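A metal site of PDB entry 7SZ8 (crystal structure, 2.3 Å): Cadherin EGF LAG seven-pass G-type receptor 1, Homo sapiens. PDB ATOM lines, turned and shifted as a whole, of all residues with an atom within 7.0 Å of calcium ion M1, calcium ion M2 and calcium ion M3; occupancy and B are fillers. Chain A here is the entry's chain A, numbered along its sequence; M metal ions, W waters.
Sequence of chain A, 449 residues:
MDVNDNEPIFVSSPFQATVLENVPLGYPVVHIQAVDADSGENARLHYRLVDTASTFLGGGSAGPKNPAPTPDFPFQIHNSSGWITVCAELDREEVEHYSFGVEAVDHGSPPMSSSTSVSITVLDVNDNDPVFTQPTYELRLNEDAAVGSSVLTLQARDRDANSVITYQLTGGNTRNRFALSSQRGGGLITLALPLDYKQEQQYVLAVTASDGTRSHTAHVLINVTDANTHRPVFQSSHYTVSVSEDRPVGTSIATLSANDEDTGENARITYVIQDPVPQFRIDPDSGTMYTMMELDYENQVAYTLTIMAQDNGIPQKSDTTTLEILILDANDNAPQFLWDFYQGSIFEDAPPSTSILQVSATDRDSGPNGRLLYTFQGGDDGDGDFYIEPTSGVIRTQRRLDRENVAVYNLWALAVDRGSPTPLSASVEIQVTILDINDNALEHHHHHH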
ATOM      1  N   GLU A  21      -0.525  16.265 -11.291  1.00  0.00           N
ATOM      2  CA  GLU A  21      -0.710  15.361 -10.123  1.00  0.00           C
ATOM      3  C   GLU A  21      -1.737  14.270 -10.448  1.00  0.00           C
ATOM      4  O   GLU A  21      -1.881  13.351  -9.660  1.00  0.00           O
ATOM      5  CB  GLU A  21      -1.102  16.137  -8.871  1.00  0.00           C
ATOM      6  CG  GLU A  21      -2.526  16.717  -8.866  1.00  0.00           C
ATOM      7  CD  GLU A  21      -2.871  17.298  -7.506  1.00  0.00           C
ATOM      8  OE1 GLU A  21      -2.549  16.666  -6.450  1.00  0.00           O
ATOM      9  OE2 GLU A  21      -3.375  18.431  -7.483  1.00  0.00           O
ATOM     10  N   LEU A  90       0.002  10.359  -7.957  1.00  0.00           N
ATOM     11  CA  LEU A  90       0.732  11.563  -7.480  1.00  0.00           C
ATOM     12  C   LEU A  90      -0.243  12.410  -6.652  1.00  0.00           C
ATOM     13  O   LEU A  90      -1.468  12.183  -6.772  1.00  0.00           O
ATOM     14  CB  LEU A  90       1.208  12.344  -8.696  1.00  0.00           C
ATOM     15  CG  LEU A  90       2.223  11.657  -9.591  1.00  0.00           C
ATOM     16  CD1 LEU A  90       2.776  12.660 -10.600  1.00  0.00           C
ATOM     17  CD2 LEU A  90       3.326  11.042  -8.771  1.00  0.00           C
ATOM     18  N   ASP A  91       0.269  13.350  -5.847  1.00  0.00           N
ATOM     19  CA  ASP A  91      -0.574  14.276  -5.055  1.00  0.00           C
ATOM     20  C   ASP A  91       0.245  15.514  -4.720  1.00  0.00           C
ATOM     21  O   ASP A  91       1.059  15.439  -3.833  1.00  0.00           O
ATOM     22  CB  ASP A  91      -1.116  13.559  -3.810  1.00  0.00           C
ATOM     23  CG  ASP A  91      -1.998  14.411  -2.900  1.00  0.00           C
ATOM     24  OD1 ASP A  91      -2.364  15.511  -3.286  1.00  0.00           O
ATOM     25  OD2 ASP A  91      -2.334  13.930  -1.829  1.00  0.00           O
ATOM     26  N   ARG A  92       0.008  16.633  -5.401  1.00  0.00           N
ATOM     27  CA  ARG A  92       0.812  17.861  -5.183  1.00  0.00           C
ATOM     28  C   ARG A  92       0.651  18.333  -3.727  1.00  0.00           C
ATOM     29  O   ARG A  92       1.596  18.884  -3.193  1.00  0.00           O
ATOM     30  CB  ARG A  92       0.411  18.992  -6.144  1.00  0.00           C
ATOM     31  CG  ARG A  92       1.449  20.108  -6.138  1.00  0.00           C
ATOM     32  CD  ARG A  92       0.881  21.474  -6.381  1.00  0.00           C
ATOM     33  NE  ARG A  92      -0.232  21.721  -5.476  1.00  0.00           N
ATOM     34  CZ  ARG A  92      -0.185  22.421  -4.367  1.00  0.00           C
ATOM     35  NH1 ARG A  92       0.953  22.965  -3.951  1.00  0.00           N
ATOM     36  NH2 ARG A  92      -1.301  22.535  -3.661  1.00  0.00           N
ATOM     37  N   GLU A  93      -0.489  18.042  -3.111  1.00  0.00           N
ATOM     38  CA  GLU A  93      -0.785  18.438  -1.714  1.00  0.00           C
ATOM     39  C   GLU A  93      -0.021  17.553  -0.713  1.00  0.00           C
ATOM     40  O   GLU A  93      -0.001  17.919   0.451  1.00  0.00           O
ATOM     41  CB  GLU A  93      -2.287  18.421  -1.451  1.00  0.00           C
ATOM     42  CG  GLU A  93      -2.997  19.578  -2.108  1.00  0.00           C
ATOM     43  CD  GLU A  93      -3.281  19.378  -3.597  1.00  0.00           C
ATOM     44  OE1 GLU A  93      -3.771  18.284  -3.974  1.00  0.00           O
ATOM     45  OE2 GLU A  93      -3.020  20.335  -4.376  1.00  0.00           O
ATOM     46  N   GLU A  94       0.628  16.477  -1.175  1.00  0.00           N
ATOM     47  CA  GLU A  94       1.532  15.630  -0.360  1.00  0.00           C
ATOM     48  C   GLU A  94       2.989  16.028  -0.616  1.00  0.00           C
ATOM     49  O   GLU A  94       3.715  16.202   0.328  1.00  0.00           O
ATOM     50  CB  GLU A  94       1.355  14.149  -0.709  1.00  0.00           C
ATOM     51  CG  GLU A  94       2.013  13.205   0.301  1.00  0.00           C
ATOM     52  CD  GLU A  94       1.226  13.017   1.592  1.00  0.00           C
ATOM     53  OE1 GLU A  94       1.861  12.989   2.669  1.00  0.00           O
ATOM     54  OE2 GLU A  94      -0.005  12.870   1.520  1.00  0.00           O
ATOM     55  N   LEU A 123       2.569  19.295 -10.862  1.00  0.00           N
ATOM     56  CA  LEU A 123       1.708  20.468 -11.220  1.00  0.00           C
ATOM     57  C   LEU A 123       0.331  20.312 -10.589  1.00  0.00           C
ATOM     58  O   LEU A 123      -0.191  19.134 -10.557  1.00  0.00           O
ATOM     59  CB  LEU A 123       1.631  20.595 -12.748  1.00  0.00           C
ATOM     60  CG  LEU A 123       2.946  20.996 -13.422  1.00  0.00           C
ATOM     61  CD1 LEU A 123       2.780  21.147 -14.920  1.00  0.00           C
ATOM     62  CD2 LEU A 123       3.524  22.271 -12.809  1.00  0.00           C
ATOM     63  N   ASP A 124      -0.230  21.413 -10.100  1.00  0.00           N
ATOM     64  CA  ASP A 124      -1.490  21.461  -9.321  1.00  0.00           C
ATOM     65  C   ASP A 124      -2.673  21.303 -10.259  1.00  0.00           C
ATOM     66  O   ASP A 124      -2.655  21.937 -11.315  1.00  0.00           O
ATOM     67  CB  ASP A 124      -1.750  22.777  -8.599  1.00  0.00           C
ATOM     68  CG  ASP A 124      -2.880  22.721  -7.575  1.00  0.00           C
ATOM     69  OD1 ASP A 124      -2.811  21.824  -6.707  1.00  0.00           O
ATOM     70  OD2 ASP A 124      -3.779  23.624  -7.603  1.00  0.00           O
ATOM     71  N   VAL A 125      -3.634  20.462  -9.836  1.00  0.00           N
ATOM     72  CA  VAL A 125      -5.015  20.304 -10.386  1.00  0.00           C
ATOM     73  C   VAL A 125      -5.996  20.678  -9.251  1.00  0.00           C
ATOM     74  O   VAL A 125      -5.615  20.633  -8.033  1.00  0.00           O
ATOM     75  CB  VAL A 125      -5.205  18.847 -10.846  1.00  0.00           C
ATOM     76  CG1 VAL A 125      -6.657  18.448 -10.933  1.00  0.00           C
ATOM     77  CG2 VAL A 125      -4.478  18.556 -12.146  1.00  0.00           C
ATOM     78  N   ASN A 126      -7.223  21.060  -9.601  1.00  0.00           N
ATOM     79  CA  ASN A 126      -8.252  21.484  -8.624  1.00  0.00           C
ATOM     80  C   ASN A 126      -9.022  20.241  -8.135  1.00  0.00           C
ATOM     81  O   ASN A 126     -10.071  19.909  -8.718  1.00  0.00           O
ATOM     82  CB  ASN A 126      -9.164  22.572  -9.210  1.00  0.00           C
ATOM     83  CG  ASN A 126     -10.060  23.125  -8.132  1.00  0.00           C
ATOM     84  OD1 ASN A 126      -9.787  22.975  -6.953  1.00  0.00           O
ATOM     85  ND2 ASN A 126     -11.123  23.807  -8.526  1.00  0.00           N
ATOM     86  N   ASP A 127      -8.478  19.562  -7.131  1.00  0.00           N
ATOM     87  CA  ASP A 127      -8.983  18.250  -6.646  1.00  0.00           C
ATOM     88  C   ASP A 127      -9.340  18.404  -5.165  1.00  0.00           C
ATOM     89  O   ASP A 127      -9.693  17.381  -4.570  1.00  0.00           O
ATOM     90  CB  ASP A 127      -8.022  17.086  -7.000  1.00  0.00           C
ATOM     91  CG  ASP A 127      -6.600  17.177  -6.453  1.00  0.00           C
ATOM     92  OD1 ASP A 127      -6.253  18.224  -5.900  1.00  0.00           O
ATOM     93  OD2 ASP A 127      -5.830  16.143  -6.548  1.00  0.00           O
ATOM     94  N   ASN A 128      -9.335  19.623  -4.609  1.00  0.00           N
ATOM     95  CA  ASN A 128      -9.802  19.839  -3.221  1.00  0.00           C
ATOM     96  C   ASN A 128     -10.887  20.917  -3.170  1.00  0.00           C
ATOM     97  O   ASN A 128     -10.694  21.996  -3.803  1.00  0.00           O
ATOM     98  CB  ASN A 128      -8.677  20.226  -2.264  1.00  0.00           C
ATOM     99  CG  ASN A 128      -7.750  19.057  -2.004  1.00  0.00           C
ATOM    100  OD1 ASN A 128      -7.860  18.388  -0.984  1.00  0.00           O
ATOM    101  ND2 ASN A 128      -6.828  18.818  -2.920  1.00  0.00           N
ATOM    102  N   ASP A 129     -11.947  20.621  -2.409  1.00  0.00           N
ATOM    103  CA  ASP A 129     -13.017  21.570  -2.012  1.00  0.00           C
ATOM    104  C   ASP A 129     -12.436  22.594  -1.021  1.00  0.00           C
ATOM    105  O   ASP A 129     -11.608  22.232  -0.177  1.00  0.00           O
ATOM    106  CB  ASP A 129     -14.220  20.873  -1.365  1.00  0.00           C
ATOM    107  CG  ASP A 129     -14.968  19.871  -2.235  1.00  0.00           C
ATOM    108  OD1 ASP A 129     -14.657  19.744  -3.449  1.00  0.00           O
ATOM    109  OD2 ASP A 129     -15.859  19.183  -1.694  1.00  0.00           O
ATOM    110  N   PRO A 130     -12.890  23.864  -1.033  1.00  0.00           N
ATOM    111  CA  PRO A 130     -12.629  24.790   0.078  1.00  0.00           C
ATOM    112  C   PRO A 130     -13.278  24.262   1.357  1.00  0.00           C
ATOM    113  O   PRO A 130     -14.350  23.662   1.277  1.00  0.00           O
ATOM    114  CB  PRO A 130     -13.307  26.117  -0.324  1.00  0.00           C
ATOM    115  CG  PRO A 130     -13.512  25.985  -1.829  1.00  0.00           C
ATOM    116  CD  PRO A 130     -13.732  24.493  -2.052  1.00  0.00           C
ATOM    117  N   ASP A 158      -8.225  26.397   0.938  1.00  0.00           N
ATOM    118  CA  ASP A 158      -8.148  25.441  -0.191  1.00  0.00           C
ATOM    119  C   ASP A 158      -6.695  24.995  -0.239  1.00  0.00           C
ATOM    120  O   ASP A 158      -5.818  25.871  -0.430  1.00  0.00           O
ATOM    121  CB  ASP A 158      -8.580  26.090  -1.505  1.00  0.00           C
ATOM    122  CG  ASP A 158      -9.095  25.105  -2.553  1.00  0.00           C
ATOM    123  OD1 ASP A 158      -8.446  24.081  -2.778  1.00  0.00           O
ATOM    124  OD2 ASP A 158     -10.156  25.401  -3.177  1.00  0.00           O
ATOM    125  N   ARG A 159      -6.459  23.687  -0.081  1.00  0.00           N
ATOM    126  CA  ARG A 159      -5.115  23.072  -0.128  1.00  0.00           C
ATOM    127  C   ARG A 159      -4.523  23.137  -1.528  1.00  0.00           C
ATOM    128  O   ARG A 159      -3.361  22.914  -1.656  1.00  0.00           O
ATOM    129  CB  ARG A 159      -5.194  21.623   0.346  1.00  0.00           C
ATOM    130  CG  ARG A 159      -5.530  21.489   1.827  1.00  0.00           C
ATOM    131  CD  ARG A 159      -5.961  20.079   2.191  1.00  0.00           C
ATOM    132  NE  ARG A 159      -4.860  19.128   2.144  1.00  0.00           N
ATOM    133  CZ  ARG A 159      -4.823  18.012   1.390  1.00  0.00           C
ATOM    134  NH1 ARG A 159      -5.812  17.665   0.578  1.00  0.00           N
ATOM    135  NH2 ARG A 159      -3.767  17.221   1.503  1.00  0.00           N
ATOM    136  N   ASP A 160      -5.301  23.415  -2.577  1.00  0.00           N
ATOM    137  CA  ASP A 160      -4.750  23.674  -3.927  1.00  0.00           C
ATOM    138  C   ASP A 160      -3.985  25.018  -3.878  1.00  0.00           C
ATOM    139  O   ASP A 160      -4.472  25.974  -3.273  1.00  0.00           O
ATOM    140  CB  ASP A 160      -5.873  23.490  -4.946  1.00  0.00           C
ATOM    141  CG  ASP A 160      -6.544  22.102  -4.971  1.00  0.00           C
ATOM    142  OD1 ASP A 160      -5.797  21.089  -5.078  1.00  0.00           O
ATOM    143  OD2 ASP A 160      -7.804  22.038  -4.917  1.00  0.00           O
ATOM    144  N   ALA A 161      -2.806  25.148  -4.489  1.00  0.00           N
ATOM    145  CA  ALA A 161      -2.059  26.434  -4.592  1.00  0.00           C
ATOM    146  C   ALA A 161      -2.802  27.408  -5.535  1.00  0.00           C
ATOM    147  O   ALA A 161      -2.765  28.600  -5.305  1.00  0.00           O
ATOM    148  CB  ALA A 161      -0.653  26.187  -5.083  1.00  0.00           C
ATOM    149  N   ASN A 162      -3.533  26.901  -6.516  1.00  0.00           N
ATOM    150  CA  ASN A 162      -4.067  27.720  -7.642  1.00  0.00           C
ATOM    151  C   ASN A 162      -5.566  27.982  -7.437  1.00  0.00           C
ATOM    152  O   ASN A 162      -6.278  28.222  -8.455  1.00  0.00           O
ATOM    153  CB  ASN A 162      -3.785  27.048  -8.989  1.00  0.00           C
ATOM    154  CG  ASN A 162      -2.308  26.747  -9.193  1.00  0.00           C
ATOM    155  OD1 ASN A 162      -1.427  27.499  -8.766  1.00  0.00           O
ATOM    156  ND2 ASN A 162      -2.042  25.665  -9.880  1.00  0.00           N
ATOM    157  N   SER A 163      -6.011  28.013  -6.191  1.00  0.00           N
ATOM    158  CA  SER A 163      -7.439  28.159  -5.802  1.00  0.00           C
ATOM    159  C   SER A 163      -7.582  29.467  -5.028  1.00  0.00           C
ATOM    160  O   SER A 163      -7.006  29.538  -3.967  1.00  0.00           O
ATOM    161  CB  SER A 163      -7.926  26.920  -5.034  1.00  0.00           C
ATOM    162  OG  SER A 163      -8.163  25.792  -5.904  1.00  0.00           O
ATOM    163  N   VAL A 164      -8.241  30.473  -5.643  1.00  0.00           N
ATOM    164  CA  VAL A 164      -8.805  31.741  -5.093  1.00  0.00           C
ATOM    165  C   VAL A 164     -10.205  31.463  -4.538  1.00  0.00           C
ATOM    166  O   VAL A 164     -11.045  30.899  -5.293  1.00  0.00           O
ATOM    167  CB  VAL A 164      -8.958  32.819  -6.192  1.00  0.00           C
ATOM    168  CG1 VAL A 164      -9.201  34.189  -5.598  1.00  0.00           C
ATOM    169  CG2 VAL A 164      -7.809  32.842  -7.199  1.00  0.00           C
ATOM    170  N   ASP A 211     -13.975  28.008  -5.125  1.00  0.00           N
ATOM    171  CA  ASP A 211     -12.699  28.229  -5.835  1.00  0.00           C
ATOM    172  C   ASP A 211     -12.999  28.539  -7.319  1.00  0.00           C
ATOM    173  O   ASP A 211     -12.057  28.645  -8.096  1.00  0.00           O
ATOM    174  CB  ASP A 211     -11.772  27.042  -5.678  1.00  0.00           C
ATOM    175  CG  ASP A 211     -12.302  25.738  -6.237  1.00  0.00           C
ATOM    176  OD1 ASP A 211     -13.202  25.813  -7.091  1.00  0.00           O
ATOM    177  OD2 ASP A 211     -11.797  24.654  -5.817  1.00  0.00           O
ATOM    178  N   THR A 213     -14.997  26.495  -9.104  1.00  0.00           N
ATOM    179  CA  THR A 213     -15.610  25.246  -9.636  1.00  0.00           C
ATOM    180  C   THR A 213     -16.140  24.371  -8.479  1.00  0.00           C
ATOM    181  O   THR A 213     -17.212  23.827  -8.657  1.00  0.00           O
ATOM    182  CB  THR A 213     -14.702  24.523 -10.640  1.00  0.00           C
ATOM    183  OG1 THR A 213     -13.770  23.694  -9.963  1.00  0.00           O
ATOM    184  CG2 THR A 213     -13.867  25.422 -11.507  1.00  0.00           C
ATOM    185  N   ARG A 214     -15.414  24.260  -7.356  1.00  0.00           N
ATOM    186  CA  ARG A 214     -15.797  23.464  -6.161  1.00  0.00           C
ATOM    187  C   ARG A 214     -16.191  24.378  -5.010  1.00  0.00           C
ATOM    188  O   ARG A 214     -15.545  25.487  -4.834  1.00  0.00           O
ATOM    189  CB  ARG A 214     -14.625  22.640  -5.650  1.00  0.00           C
ATOM    190  CG  ARG A 214     -14.128  21.628  -6.664  1.00  0.00           C
ATOM    191  CD  ARG A 214     -12.774  21.156  -6.232  1.00  0.00           C
ATOM    192  NE  ARG A 214     -12.497  19.954  -6.979  1.00  0.00           N
ATOM    193  CZ  ARG A 214     -12.862  18.746  -6.619  1.00  0.00           C
ATOM    194  NH1 ARG A 214     -13.521  18.533  -5.493  1.00  0.00           N
ATOM    195  NH2 ARG A 214     -12.495  17.747  -7.398  1.00  0.00           N
HETATM  196 CA    CA M   1      -4.476  19.919  -6.082  1.00  0.00          CA
HETATM  197 CA    CA M   2      -4.001  16.174  -4.927  1.00  0.00          CA
HETATM  198 CA    CA M   3      -9.690  23.832  -4.855  1.00  0.00          CA
HETATM  199  O   HOH W   1      -5.759  15.844  -3.236  1.00  0.00           O
HETATM  200  O   HOH W   2      -4.346  13.759  -5.414  1.00  0.00           O
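The nearest printed residue that does not touch calcium ion M3 is Arg 214 (4.3 Å).
Within 4 Å of calcium ion M2: Glu 21, Asp 91, Glu 93 and Asp 127.
Calcium ion M1 is bound by the side-chain carboxylate (OD1) of Asp 160, the side-chain carboxylate (OE2) of Glu 93, the side-chain carboxylate (OE2) of Glu 21, the backbone carbonyl oxygen (O) of Val 125, the side-chain carboxylate (OD1) of Asp 127, the side-chain carboxylate (OD1) of Asp 124 and the side-chain carboxylate (OE1) of Glu 93.
Calcium ion M1 has seven donor atoms within binding distance.
OD1 of Asn 126 is bound to calcium ion M3, at 2.3 Å.
O of Asn 128 is bound to calcium ion M3 (2.3 Å).
OD2 of Asp 158 is bound to calcium ion M3 (2.3 Å).
Calcium ion M3 is bound by OD1 of Asp 158, at 2.4 Å.
Calcium ion M3 is bound by OD2 of Asp 211 (2.5 Å).
The side-chain carboxylate (OD2) of Asp 160 is bound to calcium ion M3.
Calcium ion M3 is bound by the side-chain hydroxyl (OG) of Ser 163 (2.7 Å).
Calcium ion M2 is bound by the side-chain carboxylate (OE1) of Glu 21 (2.2 Å), the side-chain carboxylate (OE1) of Glu 93 (2.3 Å), the side-chain carboxylate (OD1) of Asp 91 (2.4 Å), the side-chain carboxylate (OD2) of Asp 127 (2.4 Å), water W1 (2.5 Å) and water W2 (2.5 Å).
Calcium ion M2 has six donor atoms within binding distance.
Within 4 Å of calcium ion M1: Glu 21, Glu 93, Asp 124, Val 125, Asp 127 and Asp 160.
The nearest printed residue that does not touch calcium ion M1 is Asn 128 (4.1 Å).
The backbone NH (N) of Arg 92 sits close to the side-chain carboxylate (OE1) of Glu 21 (2.8 Å).
The backbone carbonyl oxygen (O) of Asn 126 sits at hydrogen-bond distance from the guanidinium group (NE) of Arg 214, 3.0 Å away.
The side-chain amide nitrogen (ND2) of Asn 126 lies within hydrogen-bond range of the side-chain hydroxyl (OG1) of Thr 213 (3.0 Å).
ND2 of Asn 128 lies close to OD1 of Asp 127 (3.1 Å).
The guanidinium group (NH1) of Arg 159 lies within hydrogen-bond range of the side-chain amide oxygen (OD1) of Asn 128 (2.7 Å).
OD1 of Asp 211 is in hydrogen-bond range of N of Arg 214 (2.7 Å).
The side-chain carboxylate of Asp 124 sits close to the guanidinium group of Arg 92 (2.9 Å).
OD2 of Asp 124 sits at hydrogen-bond distance from N of Asn 162 (3.5 Å).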
